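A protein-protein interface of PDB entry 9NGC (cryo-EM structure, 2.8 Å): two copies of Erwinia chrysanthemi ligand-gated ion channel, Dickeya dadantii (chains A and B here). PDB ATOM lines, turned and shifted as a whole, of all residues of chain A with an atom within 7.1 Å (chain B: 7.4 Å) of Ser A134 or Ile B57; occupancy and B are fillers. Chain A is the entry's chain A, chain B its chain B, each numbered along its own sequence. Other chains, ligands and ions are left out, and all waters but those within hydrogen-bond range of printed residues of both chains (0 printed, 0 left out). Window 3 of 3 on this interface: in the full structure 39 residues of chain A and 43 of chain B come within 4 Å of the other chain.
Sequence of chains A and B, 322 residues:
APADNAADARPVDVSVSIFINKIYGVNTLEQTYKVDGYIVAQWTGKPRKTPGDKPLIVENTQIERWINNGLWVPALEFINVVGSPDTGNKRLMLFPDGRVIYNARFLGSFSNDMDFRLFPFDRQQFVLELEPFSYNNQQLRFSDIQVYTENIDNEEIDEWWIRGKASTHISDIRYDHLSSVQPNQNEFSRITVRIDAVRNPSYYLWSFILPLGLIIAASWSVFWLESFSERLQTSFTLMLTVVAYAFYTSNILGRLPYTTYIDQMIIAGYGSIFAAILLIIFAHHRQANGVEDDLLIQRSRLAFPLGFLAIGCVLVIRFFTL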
ATOM      1  N   TRP A  72     -19.858  12.268  -1.105  1.00  0.00           N
ATOM      2  CA  TRP A  72     -18.534  12.407  -0.507  1.00  0.00           C
ATOM      3  C   TRP A  72     -17.503  11.885  -1.500  1.00  0.00           C
ATOM      4  O   TRP A  72     -17.322  10.675  -1.648  1.00  0.00           O
ATOM      5  CB  TRP A  72     -18.458  11.660   0.820  1.00  0.00           C
ATOM      6  CG  TRP A  72     -17.167  11.870   1.530  1.00  0.00           C
ATOM      7  CD1 TRP A  72     -16.809  12.956   2.267  1.00  0.00           C
ATOM      8  CD2 TRP A  72     -16.051  10.975   1.564  1.00  0.00           C
ATOM      9  NE1 TRP A  72     -15.541  12.793   2.763  1.00  0.00           N
ATOM     10  CE2 TRP A  72     -15.054  11.583   2.344  1.00  0.00           C
ATOM     11  CE3 TRP A  72     -15.800   9.717   1.011  1.00  0.00           C
ATOM     12  CZ2 TRP A  72     -13.826  10.980   2.586  1.00  0.00           C
ATOM     13  CZ3 TRP A  72     -14.582   9.120   1.251  1.00  0.00           C
ATOM     14  CH2 TRP A  72     -13.611   9.752   2.029  1.00  0.00           C
ATOM     15  N   PRO A  74     -13.576  12.460  -1.966  1.00  0.00           N
ATOM     16  CA  PRO A  74     -12.365  13.096  -1.442  1.00  0.00           C
ATOM     17  C   PRO A  74     -11.416  13.521  -2.550  1.00  0.00           C
ATOM     18  O   PRO A  74     -11.393  12.945  -3.639  1.00  0.00           O
ATOM     19  CB  PRO A  74     -11.740  12.003  -0.574  1.00  0.00           C
ATOM     20  CG  PRO A  74     -12.218  10.738  -1.180  1.00  0.00           C
ATOM     21  CD  PRO A  74     -13.604  11.016  -1.685  1.00  0.00           C
ATOM     22  N   ALA A  75     -10.621  14.544  -2.252  1.00  0.00           N
ATOM     23  CA  ALA A  75      -9.644  15.079  -3.187  1.00  0.00           C
ATOM     24  C   ALA A  75      -8.264  14.558  -2.817  1.00  0.00           C
ATOM     25  O   ALA A  75      -7.751  14.864  -1.737  1.00  0.00           O
ATOM     26  CB  ALA A  75      -9.658  16.606  -3.181  1.00  0.00           C
ATOM     27  N   GLU A  77      -4.346  14.619  -3.649  1.00  0.00           N
ATOM     28  CA  GLU A  77      -3.356  15.481  -4.270  1.00  0.00           C
ATOM     29  C   GLU A  77      -2.027  14.753  -4.402  1.00  0.00           C
ATOM     30  O   GLU A  77      -1.742  13.792  -3.684  1.00  0.00           O
ATOM     31  CB  GLU A  77      -3.170  16.768  -3.462  1.00  0.00           C
ATOM     32  CG  GLU A  77      -2.554  16.550  -2.094  1.00  0.00           C
ATOM     33  CD  GLU A  77      -2.106  17.838  -1.445  1.00  0.00           C
ATOM     34  OE1 GLU A  77      -2.297  18.908  -2.056  1.00  0.00           O
ATOM     35  OE2 GLU A  77      -1.560  17.779  -0.325  1.00  0.00           O
ATOM     36  N   GLU A 131      -1.474  11.730  -1.642  1.00  0.00           N
ATOM     37  CA  GLU A 131      -1.922  11.995  -0.284  1.00  0.00           C
ATOM     38  C   GLU A 131      -3.266  12.697  -0.328  1.00  0.00           C
ATOM     39  O   GLU A 131      -3.492  13.503  -1.240  1.00  0.00           O
ATOM     40  CB  GLU A 131      -0.899  12.862   0.454  1.00  0.00           C
ATOM     41  CG  GLU A 131      -0.917  12.734   1.954  1.00  0.00           C
ATOM     42  CD  GLU A 131       0.387  13.162   2.575  1.00  0.00           C
ATOM     43  OE1 GLU A 131       1.432  13.054   1.903  1.00  0.00           O
ATOM     44  OE2 GLU A 131       0.371  13.605   3.736  1.00  0.00           O
ATOM     45  N   PRO A 132      -4.180  12.411   0.597  1.00  0.00           N
ATOM     46  CA  PRO A 132      -5.382  13.241   0.721  1.00  0.00           C
ATOM     47  C   PRO A 132      -5.028  14.641   1.190  1.00  0.00           C
ATOM     48  O   PRO A 132      -4.069  14.847   1.937  1.00  0.00           O
ATOM     49  CB  PRO A 132      -6.222  12.506   1.770  1.00  0.00           C
ATOM     50  CG  PRO A 132      -5.654  11.148   1.845  1.00  0.00           C
ATOM     51  CD  PRO A 132      -4.214  11.264   1.514  1.00  0.00           C
ATOM     52  N   PHE A 133      -5.814  15.615   0.740  1.00  0.00           N
ATOM     53  CA  PHE A 133      -5.538  16.993   1.120  1.00  0.00           C
ATOM     54  C   PHE A 133      -6.055  17.333   2.510  1.00  0.00           C
ATOM     55  O   PHE A 133      -5.421  18.116   3.225  1.00  0.00           O
ATOM     56  CB  PHE A 133      -6.140  17.958   0.100  1.00  0.00           C
ATOM     57  CG  PHE A 133      -5.873  19.400   0.414  1.00  0.00           C
ATOM     58  CD1 PHE A 133      -4.604  19.927   0.268  1.00  0.00           C
ATOM     59  CD2 PHE A 133      -6.886  20.222   0.870  1.00  0.00           C
ATOM     60  CE1 PHE A 133      -4.352  21.248   0.564  1.00  0.00           C
ATOM     61  CE2 PHE A 133      -6.639  21.543   1.168  1.00  0.00           C
ATOM     62  CZ  PHE A 133      -5.371  22.056   1.014  1.00  0.00           C
ATOM     63  N   SER A 134      -7.186  16.763   2.917  1.00  0.00           N
ATOM     64  CA  SER A 134      -7.871  17.267   4.100  1.00  0.00           C
ATOM     65  C   SER A 134      -8.230  16.186   5.112  1.00  0.00           C
ATOM     66  O   SER A 134      -8.581  16.503   6.253  1.00  0.00           O
ATOM     67  CB  SER A 134      -9.133  18.017   3.675  1.00  0.00           C
ATOM     68  OG  SER A 134     -10.034  17.159   3.004  1.00  0.00           O
ATOM     69  N   TYR A 135      -8.155  14.919   4.724  1.00  0.00           N
ATOM     70  CA  TYR A 135      -8.588  13.825   5.581  1.00  0.00           C
ATOM     71  C   TYR A 135      -7.389  13.071   6.140  1.00  0.00           C
ATOM     72  O   TYR A 135      -6.504  12.649   5.390  1.00  0.00           O
ATOM     73  CB  TYR A 135      -9.511  12.878   4.816  1.00  0.00           C
ATOM     74  CG  TYR A 135     -10.754  13.565   4.309  1.00  0.00           C
ATOM     75  CD1 TYR A 135     -11.790  13.884   5.171  1.00  0.00           C
ATOM     76  CD2 TYR A 135     -10.884  13.911   2.972  1.00  0.00           C
ATOM     77  CE1 TYR A 135     -12.926  14.520   4.718  1.00  0.00           C
ATOM     78  CE2 TYR A 135     -12.015  14.546   2.509  1.00  0.00           C
ATOM     79  CZ  TYR A 135     -13.032  14.849   3.386  1.00  0.00           C
ATOM     80  OH  TYR A 135     -14.163  15.483   2.928  1.00  0.00           O
ATOM     81  N   ASN A 136      -7.377  12.898   7.459  1.00  0.00           N
ATOM     82  CA  ASN A 136      -6.288  12.242   8.169  1.00  0.00           C
ATOM     83  C   ASN A 136      -6.481  10.721   8.134  1.00  0.00           C
ATOM     84  O   ASN A 136      -7.369  10.211   7.448  1.00  0.00           O
ATOM     85  CB  ASN A 136      -6.174  12.852   9.568  1.00  0.00           C
ATOM     86  CG  ASN A 136      -7.410  12.633  10.432  1.00  0.00           C
ATOM     87  OD1 ASN A 136      -8.342  11.922  10.070  1.00  0.00           O
ATOM     88  ND2 ASN A 136      -7.423  13.282  11.583  1.00  0.00           N
ATOM     89  N   GLN A 139      -9.900   9.420   9.242  1.00  0.00           N
ATOM     90  CA  GLN A 139     -11.036   9.641   8.365  1.00  0.00           C
ATOM     91  C   GLN A 139     -10.863   9.066   6.969  1.00  0.00           C
ATOM     92  O   GLN A 139     -11.861   8.928   6.256  1.00  0.00           O
ATOM     93  CB  GLN A 139     -11.338  11.143   8.238  1.00  0.00           C
ATOM     94  CG  GLN A 139     -11.765  11.799   9.535  1.00  0.00           C
ATOM     95  CD  GLN A 139     -11.319  13.238   9.629  1.00  0.00           C
ATOM     96  OE1 GLN A 139     -10.967  13.857   8.628  1.00  0.00           O
ATOM     97  NE2 GLN A 139     -11.335  13.784  10.839  1.00  0.00           N
ATOM     98  N   LEU A 178      -0.767  21.301  11.394  1.00  0.00           N
ATOM     99  CA  LEU A 178      -2.167  21.021  11.666  1.00  0.00           C
ATOM    100  C   LEU A 178      -2.405  20.608  13.111  1.00  0.00           C
ATOM    101  O   LEU A 178      -3.507  20.164  13.443  1.00  0.00           O
ATOM    102  CB  LEU A 178      -2.679  19.934  10.721  1.00  0.00           C
ATOM    103  CG  LEU A 178      -2.681  20.289   9.235  1.00  0.00           C
ATOM    104  CD1 LEU A 178      -2.619  19.034   8.392  1.00  0.00           C
ATOM    105  CD2 LEU A 178      -3.901  21.114   8.878  1.00  0.00           C
ATOM    106  N   GLN A 182      -5.978  20.555  14.666  1.00  0.00           N
ATOM    107  CA  GLN A 182      -6.353  19.176  14.971  1.00  0.00           C
ATOM    108  C   GLN A 182      -5.409  18.706  16.066  1.00  0.00           C
ATOM    109  O   GLN A 182      -4.230  18.420  15.773  1.00  0.00           O
ATOM    110  CB  GLN A 182      -6.243  18.286  13.737  1.00  0.00           C
ATOM    111  CG  GLN A 182      -7.210  18.616  12.613  1.00  0.00           C
ATOM    112  CD  GLN A 182      -6.789  18.000  11.292  1.00  0.00           C
ATOM    113  OE1 GLN A 182      -5.673  17.507  11.154  1.00  0.00           O
ATOM    114  NE2 GLN A 182      -7.685  18.022  10.314  1.00  0.00           N
ATOM    115  N   PHE A 188      -1.338  11.847   8.280  1.00  0.00           N
ATOM    116  CA  PHE A 188      -1.966  11.643   6.980  1.00  0.00           C
ATOM    117  C   PHE A 188      -1.385  10.416   6.297  1.00  0.00           C
ATOM    118  O   PHE A 188      -0.165  10.236   6.270  1.00  0.00           O
ATOM    119  CB  PHE A 188      -1.790  12.877   6.092  1.00  0.00           C
ATOM    120  CG  PHE A 188      -2.800  13.959   6.345  1.00  0.00           C
ATOM    121  CD1 PHE A 188      -2.825  14.638   7.552  1.00  0.00           C
ATOM    122  CD2 PHE A 188      -3.720  14.305   5.373  1.00  0.00           C
ATOM    123  CE1 PHE A 188      -3.750  15.630   7.787  1.00  0.00           C
ATOM    124  CE2 PHE A 188      -4.646  15.299   5.603  1.00  0.00           C
ATOM    125  CZ  PHE A 188      -4.660  15.962   6.812  1.00  0.00           C
ATOM    126  N   LYS B  54     -19.291  17.393  15.367  1.00  0.00           N
ATOM    127  CA  LYS B  54     -18.001  17.207  14.737  1.00  0.00           C
ATOM    128  C   LYS B  54     -17.725  18.372  13.792  1.00  0.00           C
ATOM    129  O   LYS B  54     -18.660  18.928  13.209  1.00  0.00           O
ATOM    130  CB  LYS B  54     -17.976  15.879  13.962  1.00  0.00           C
ATOM    131  CG  LYS B  54     -16.635  15.485  13.357  1.00  0.00           C
ATOM    132  CD  LYS B  54     -16.684  14.091  12.758  1.00  0.00           C
ATOM    133  CE  LYS B  54     -17.493  14.072  11.475  1.00  0.00           C
ATOM    134  NZ  LYS B  54     -16.806  14.818  10.386  1.00  0.00           N
ATOM    135  N   PRO B  55     -16.466  18.800  13.671  1.00  0.00           N
ATOM    136  CA  PRO B  55     -16.128  19.838  12.689  1.00  0.00           C
ATOM    137  C   PRO B  55     -16.480  19.422  11.268  1.00  0.00           C
ATOM    138  O   PRO B  55     -16.344  18.258  10.888  1.00  0.00           O
ATOM    139  CB  PRO B  55     -14.615  20.004  12.859  1.00  0.00           C
ATOM    140  CG  PRO B  55     -14.339  19.580  14.243  1.00  0.00           C
ATOM    141  CD  PRO B  55     -15.396  18.607  14.665  1.00  0.00           C
ATOM    142  N   LEU B  56     -16.938  20.393  10.485  1.00  0.00           N
ATOM    143  CA  LEU B  56     -17.378  20.169   9.118  1.00  0.00           C
ATOM    144  C   LEU B  56     -16.298  20.638   8.156  1.00  0.00           C
ATOM    145  O   LEU B  56     -15.837  21.779   8.243  1.00  0.00           O
ATOM    146  CB  LEU B  56     -18.691  20.904   8.845  1.00  0.00           C
ATOM    147  CG  LEU B  56     -19.276  20.778   7.440  1.00  0.00           C
ATOM    148  CD1 LEU B  56     -19.787  19.372   7.200  1.00  0.00           C
ATOM    149  CD2 LEU B  56     -20.386  21.789   7.251  1.00  0.00           C
ATOM    150  N   ILE B  57     -15.899  19.756   7.245  1.00  0.00           N
ATOM    151  CA  ILE B  57     -14.855  20.044   6.270  1.00  0.00           C
ATOM    152  C   ILE B  57     -15.522  20.366   4.941  1.00  0.00           C
ATOM    153  O   ILE B  57     -16.252  19.537   4.386  1.00  0.00           O
ATOM    154  CB  ILE B  57     -13.882  18.866   6.127  1.00  0.00           C
ATOM    155  CG1 ILE B  57     -13.064  18.689   7.403  1.00  0.00           C
ATOM    156  CG2 ILE B  57     -12.965  19.072   4.938  1.00  0.00           C
ATOM    157  CD1 ILE B  57     -12.088  17.543   7.342  1.00  0.00           C
ATOM    158  N   VAL B  58     -15.274  21.568   4.433  1.00  0.00           N
ATOM    159  CA  VAL B  58     -15.784  22.009   3.141  1.00  0.00           C
ATOM    160  C   VAL B  58     -14.591  22.119   2.207  1.00  0.00           C
ATOM    161  O   VAL B  58     -13.731  22.988   2.383  1.00  0.00           O
ATOM    162  CB  VAL B  58     -16.532  23.342   3.249  1.00  0.00           C
ATOM    163  CG1 VAL B  58     -17.059  23.763   1.896  1.00  0.00           C
ATOM    164  CG2 VAL B  58     -17.660  23.239   4.258  1.00  0.00           C
ATOM    165  N   GLU B  59     -14.538  21.249   1.204  1.00  0.00           N
ATOM    166  CA  GLU B  59     -13.399  21.189   0.300  1.00  0.00           C
ATOM    167  C   GLU B  59     -13.541  22.262  -0.775  1.00  0.00           C
ATOM    168  O   GLU B  59     -14.397  23.144  -0.700  1.00  0.00           O
ATOM    169  CB  GLU B  59     -13.275  19.795  -0.303  1.00  0.00           C
ATOM    170  CG  GLU B  59     -12.674  18.762   0.627  1.00  0.00           C
ATOM    171  CD  GLU B  59     -11.204  18.527   0.359  1.00  0.00           C
ATOM    172  OE1 GLU B  59     -10.551  19.425  -0.212  1.00  0.00           O
ATOM    173  OE2 GLU B  59     -10.702  17.442   0.712  1.00  0.00           O
ATOM    174  N   GLN B  62     -16.762  24.101  -3.210  1.00  0.00           N
ATOM    175  CA  GLN B  62     -17.921  24.064  -2.331  1.00  0.00           C
ATOM    176  C   GLN B  62     -17.901  25.192  -1.318  1.00  0.00           C
ATOM    177  O   GLN B  62     -18.912  25.411  -0.646  1.00  0.00           O
ATOM    178  CB  GLN B  62     -18.003  22.727  -1.584  1.00  0.00           C
ATOM    179  CG  GLN B  62     -18.353  21.540  -2.456  1.00  0.00           C
ATOM    180  CD  GLN B  62     -19.833  21.449  -2.736  1.00  0.00           C
ATOM    181  OE1 GLN B  62     -20.650  21.448  -1.818  1.00  0.00           O
ATOM    182  NE2 GLN B  62     -20.188  21.375  -4.010  1.00  0.00           N
ATOM    183  N   TRP B  66     -20.990  28.431   0.505  1.00  0.00           N
ATOM    184  CA  TRP B  66     -21.034  29.050   1.826  1.00  0.00           C
ATOM    185  C   TRP B  66     -20.815  30.554   1.753  1.00  0.00           C
ATOM    186  O   TRP B  66     -21.405  31.300   2.541  1.00  0.00           O
ATOM    187  CB  TRP B  66     -19.994  28.401   2.739  1.00  0.00           C
ATOM    188  CG  TRP B  66     -20.388  27.032   3.185  1.00  0.00           C
ATOM    189  CD1 TRP B  66     -20.241  25.872   2.490  1.00  0.00           C
ATOM    190  CD2 TRP B  66     -21.009  26.683   4.425  1.00  0.00           C
ATOM    191  NE1 TRP B  66     -20.727  24.818   3.221  1.00  0.00           N
ATOM    192  CE2 TRP B  66     -21.205  25.290   4.414  1.00  0.00           C
ATOM    193  CE3 TRP B  66     -21.414  27.411   5.545  1.00  0.00           C
ATOM    194  CZ2 TRP B  66     -21.790  24.612   5.478  1.00  0.00           C
ATOM    195  CZ3 TRP B  66     -21.995  26.736   6.600  1.00  0.00           C
ATOM    196  CH2 TRP B  66     -22.177  25.351   6.560  1.00  0.00           C
ATOM    197  N   ASN B  89      -5.601  22.638  -4.167  1.00  0.00           N
ATOM    198  CA  ASN B  89      -6.745  22.337  -3.322  1.00  0.00           C
ATOM    199  C   ASN B  89      -6.837  23.347  -2.189  1.00  0.00           C
ATOM    200  O   ASN B  89      -5.823  23.814  -1.667  1.00  0.00           O
ATOM    201  CB  ASN B  89      -6.640  20.921  -2.758  1.00  0.00           C
ATOM    202  CG  ASN B  89      -6.639  19.862  -3.839  1.00  0.00           C
ATOM    203  OD1 ASN B  89      -7.692  19.445  -4.313  1.00  0.00           O
ATOM    204  ND2 ASN B  89      -5.454  19.417  -4.228  1.00  0.00           N
ATOM    205  N   LYS B  90      -8.064  23.694  -1.819  1.00  0.00           N
ATOM    206  CA  LYS B  90      -8.318  24.585  -0.700  1.00  0.00           C
ATOM    207  C   LYS B  90      -9.455  24.012   0.132  1.00  0.00           C
ATOM    208  O   LYS B  90     -10.371  23.377  -0.393  1.00  0.00           O
ATOM    209  CB  LYS B  90      -8.623  26.011  -1.183  1.00  0.00           C
ATOM    210  CG  LYS B  90      -9.894  26.157  -1.986  1.00  0.00           C
ATOM    211  CD  LYS B  90     -10.086  27.583  -2.460  1.00  0.00           C
ATOM    212  CE  LYS B  90     -11.374  27.730  -3.252  1.00  0.00           C
ATOM    213  NZ  LYS B  90     -11.579  29.122  -3.732  1.00  0.00           N
ATOM    214  N   ARG B  91      -9.374  24.225   1.441  1.00  0.00           N
ATOM    215  CA  ARG B  91     -10.262  23.579   2.395  1.00  0.00           C
ATOM    216  C   ARG B  91     -10.765  24.604   3.397  1.00  0.00           C
ATOM    217  O   ARG B  91     -10.054  25.550   3.744  1.00  0.00           O
ATOM    218  CB  ARG B  91      -9.532  22.417   3.103  1.00  0.00           C
ATOM    219  CG  ARG B  91     -10.373  21.543   4.021  1.00  0.00           C
ATOM    220  CD  ARG B  91     -10.190  21.929   5.476  1.00  0.00           C
ATOM    221  NE  ARG B  91      -8.799  21.819   5.895  1.00  0.00           N
ATOM    222  CZ  ARG B  91      -8.238  20.703   6.341  1.00  0.00           C
ATOM    223  NH1 ARG B  91      -8.939  19.595   6.503  1.00  0.00           N
ATOM    224  NH2 ARG B  91      -6.945  20.705   6.648  1.00  0.00           N
ATOM    225  N   LEU B  92     -12.000  24.416   3.845  1.00  0.00           N
ATOM    226  CA  LEU B  92     -12.617  25.242   4.871  1.00  0.00           C
ATOM    227  C   LEU B  92     -13.123  24.333   5.980  1.00  0.00           C
ATOM    228  O   LEU B  92     -13.827  23.357   5.709  1.00  0.00           O
ATOM    229  CB  LEU B  92     -13.765  26.062   4.283  1.00  0.00           C
ATOM    230  CG  LEU B  92     -14.282  27.281   5.035  1.00  0.00           C
ATOM    231  CD1 LEU B  92     -13.270  28.405   5.002  1.00  0.00           C
ATOM    232  CD2 LEU B  92     -15.584  27.718   4.411  1.00  0.00           C
ATOM    233  N   MET B  93     -12.765  24.646   7.220  1.00  0.00           N
ATOM    234  CA  MET B  93     -13.160  23.844   8.369  1.00  0.00           C
ATOM    235  C   MET B  93     -13.983  24.700   9.318  1.00  0.00           C
ATOM    236  O   MET B  93     -13.539  25.774   9.734  1.00  0.00           O
ATOM    237  CB  MET B  93     -11.936  23.268   9.082  1.00  0.00           C
ATOM    238  CG  MET B  93     -12.235  22.067   9.957  1.00  0.00           C
ATOM    239  SD  MET B  93     -10.945  20.811   9.874  1.00  0.00           S
ATOM    240  CE  MET B  93      -9.497  21.785  10.267  1.00  0.00           C
ATOM    241  N   LEU B  94     -15.174  24.220   9.661  1.00  0.00           N
ATOM    242  CA  LEU B  94     -16.126  24.959  10.479  1.00  0.00           C
ATOM    243  C   LEU B  94     -16.361  24.206  11.777  1.00  0.00           C
ATOM    244  O   LEU B  94     -16.634  23.002  11.758  1.00  0.00           O
ATOM    245  CB  LEU B  94     -17.447  25.154   9.735  1.00  0.00           C
ATOM    246  CG  LEU B  94     -17.361  25.820   8.361  1.00  0.00           C
ATOM    247  CD1 LEU B  94     -18.675  25.683   7.632  1.00  0.00           C
ATOM    248  CD2 LEU B  94     -16.979  27.278   8.492  1.00  0.00           C
ATOM    249  N   ASN B 103      -7.736  26.569   5.046  1.00  0.00           N
ATOM    250  CA  ASN B 103      -6.490  25.911   4.683  1.00  0.00           C
ATOM    251  C   ASN B 103      -6.416  25.801   3.169  1.00  0.00           C
ATOM    252  O   ASN B 103      -7.372  25.356   2.529  1.00  0.00           O
ATOM    253  CB  ASN B 103      -6.392  24.531   5.333  1.00  0.00           C
ATOM    254  CG  ASN B 103      -5.169  23.762   4.888  1.00  0.00           C
ATOM    255  OD1 ASN B 103      -4.047  24.248   4.991  1.00  0.00           O
ATOM    256  ND2 ASN B 103      -5.380  22.549   4.398  1.00  0.00           N
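The backbone carbonyl oxygen of Ser A134 is in hydrogen-bond range of the guanidinium group of Arg B91, at 3.1 Å. The side-chain hydroxyl of Ser A134 is in hydrogen-bond range of the side-chain carboxylate of Glu B59 (2.4 Å).
Ser A134 touches just these residues of chain B: Ile B57 (3.8 Å), Glu B59 (2.4 Å) and Arg B91 (3.1 Å). Of chain A, only Ser A134 (3.8 Å) comes within 4 Å of Ile B57. Of the printed residues of chain A, Asn B103 touches Phe A133 (3.4 Å). Of the printed residues of chain A, Glu B59 touches Phe A133, Ser A134 and Tyr A135. Of the printed residues of chain B, Glu A77 touches Asn B89. Of the printed residues of chain A, Lys B90 touches Phe A133 (3.9 Å). Lys B54 touches none of the printed residues of chain A. Leu B56 touches none of the printed residues of chain A. The nearest residue of chain B that does not touch Ser A134 is Asn B103 (5.8 Å). The nearest printed residue of chain B that does not touch Leu A178 is Asn B103 (4.9 Å).
Ala A75 touches Asn B89. Glu A77 touches Asn B89 (CB to ND2, 3.6 Å). CD2 of Phe A133 touches OE1 of Glu B59 (3.9 Å). CZ of Phe A133 touches O of Asn B89, 3.2 Å away. Phe A133 touches Lys B90 (CE2 to C, 3.9 Å). Phe A133 touches Arg B91. Asn B103 touches Phe A133 (ND2 to CZ, 3.4 Å). Ile B57 touches Ser A134. Tyr A135 touches Glu B59. Leu A178 touches Arg B91.
N of Glu A77 lies within hydrogen-bond range of O of Glu A131, at 2.8 Å. The backbone carbonyl oxygen of Ala A75 is in hydrogen-bond range of the backbone NH of Phe A133 (3.2 Å). NE1 of Trp A72 lies within hydrogen-bond range of OH of Tyr A135 (3.0 Å). O of Asn B103 lies within hydrogen-bond range of N of Arg B91.
No position is printed for both chains. Of the 12 pairs that touch across the chains among the printed residues, none has its exchanged pair printed and touching as well.
Among the printed residues, 12 pairs touch across the chains.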
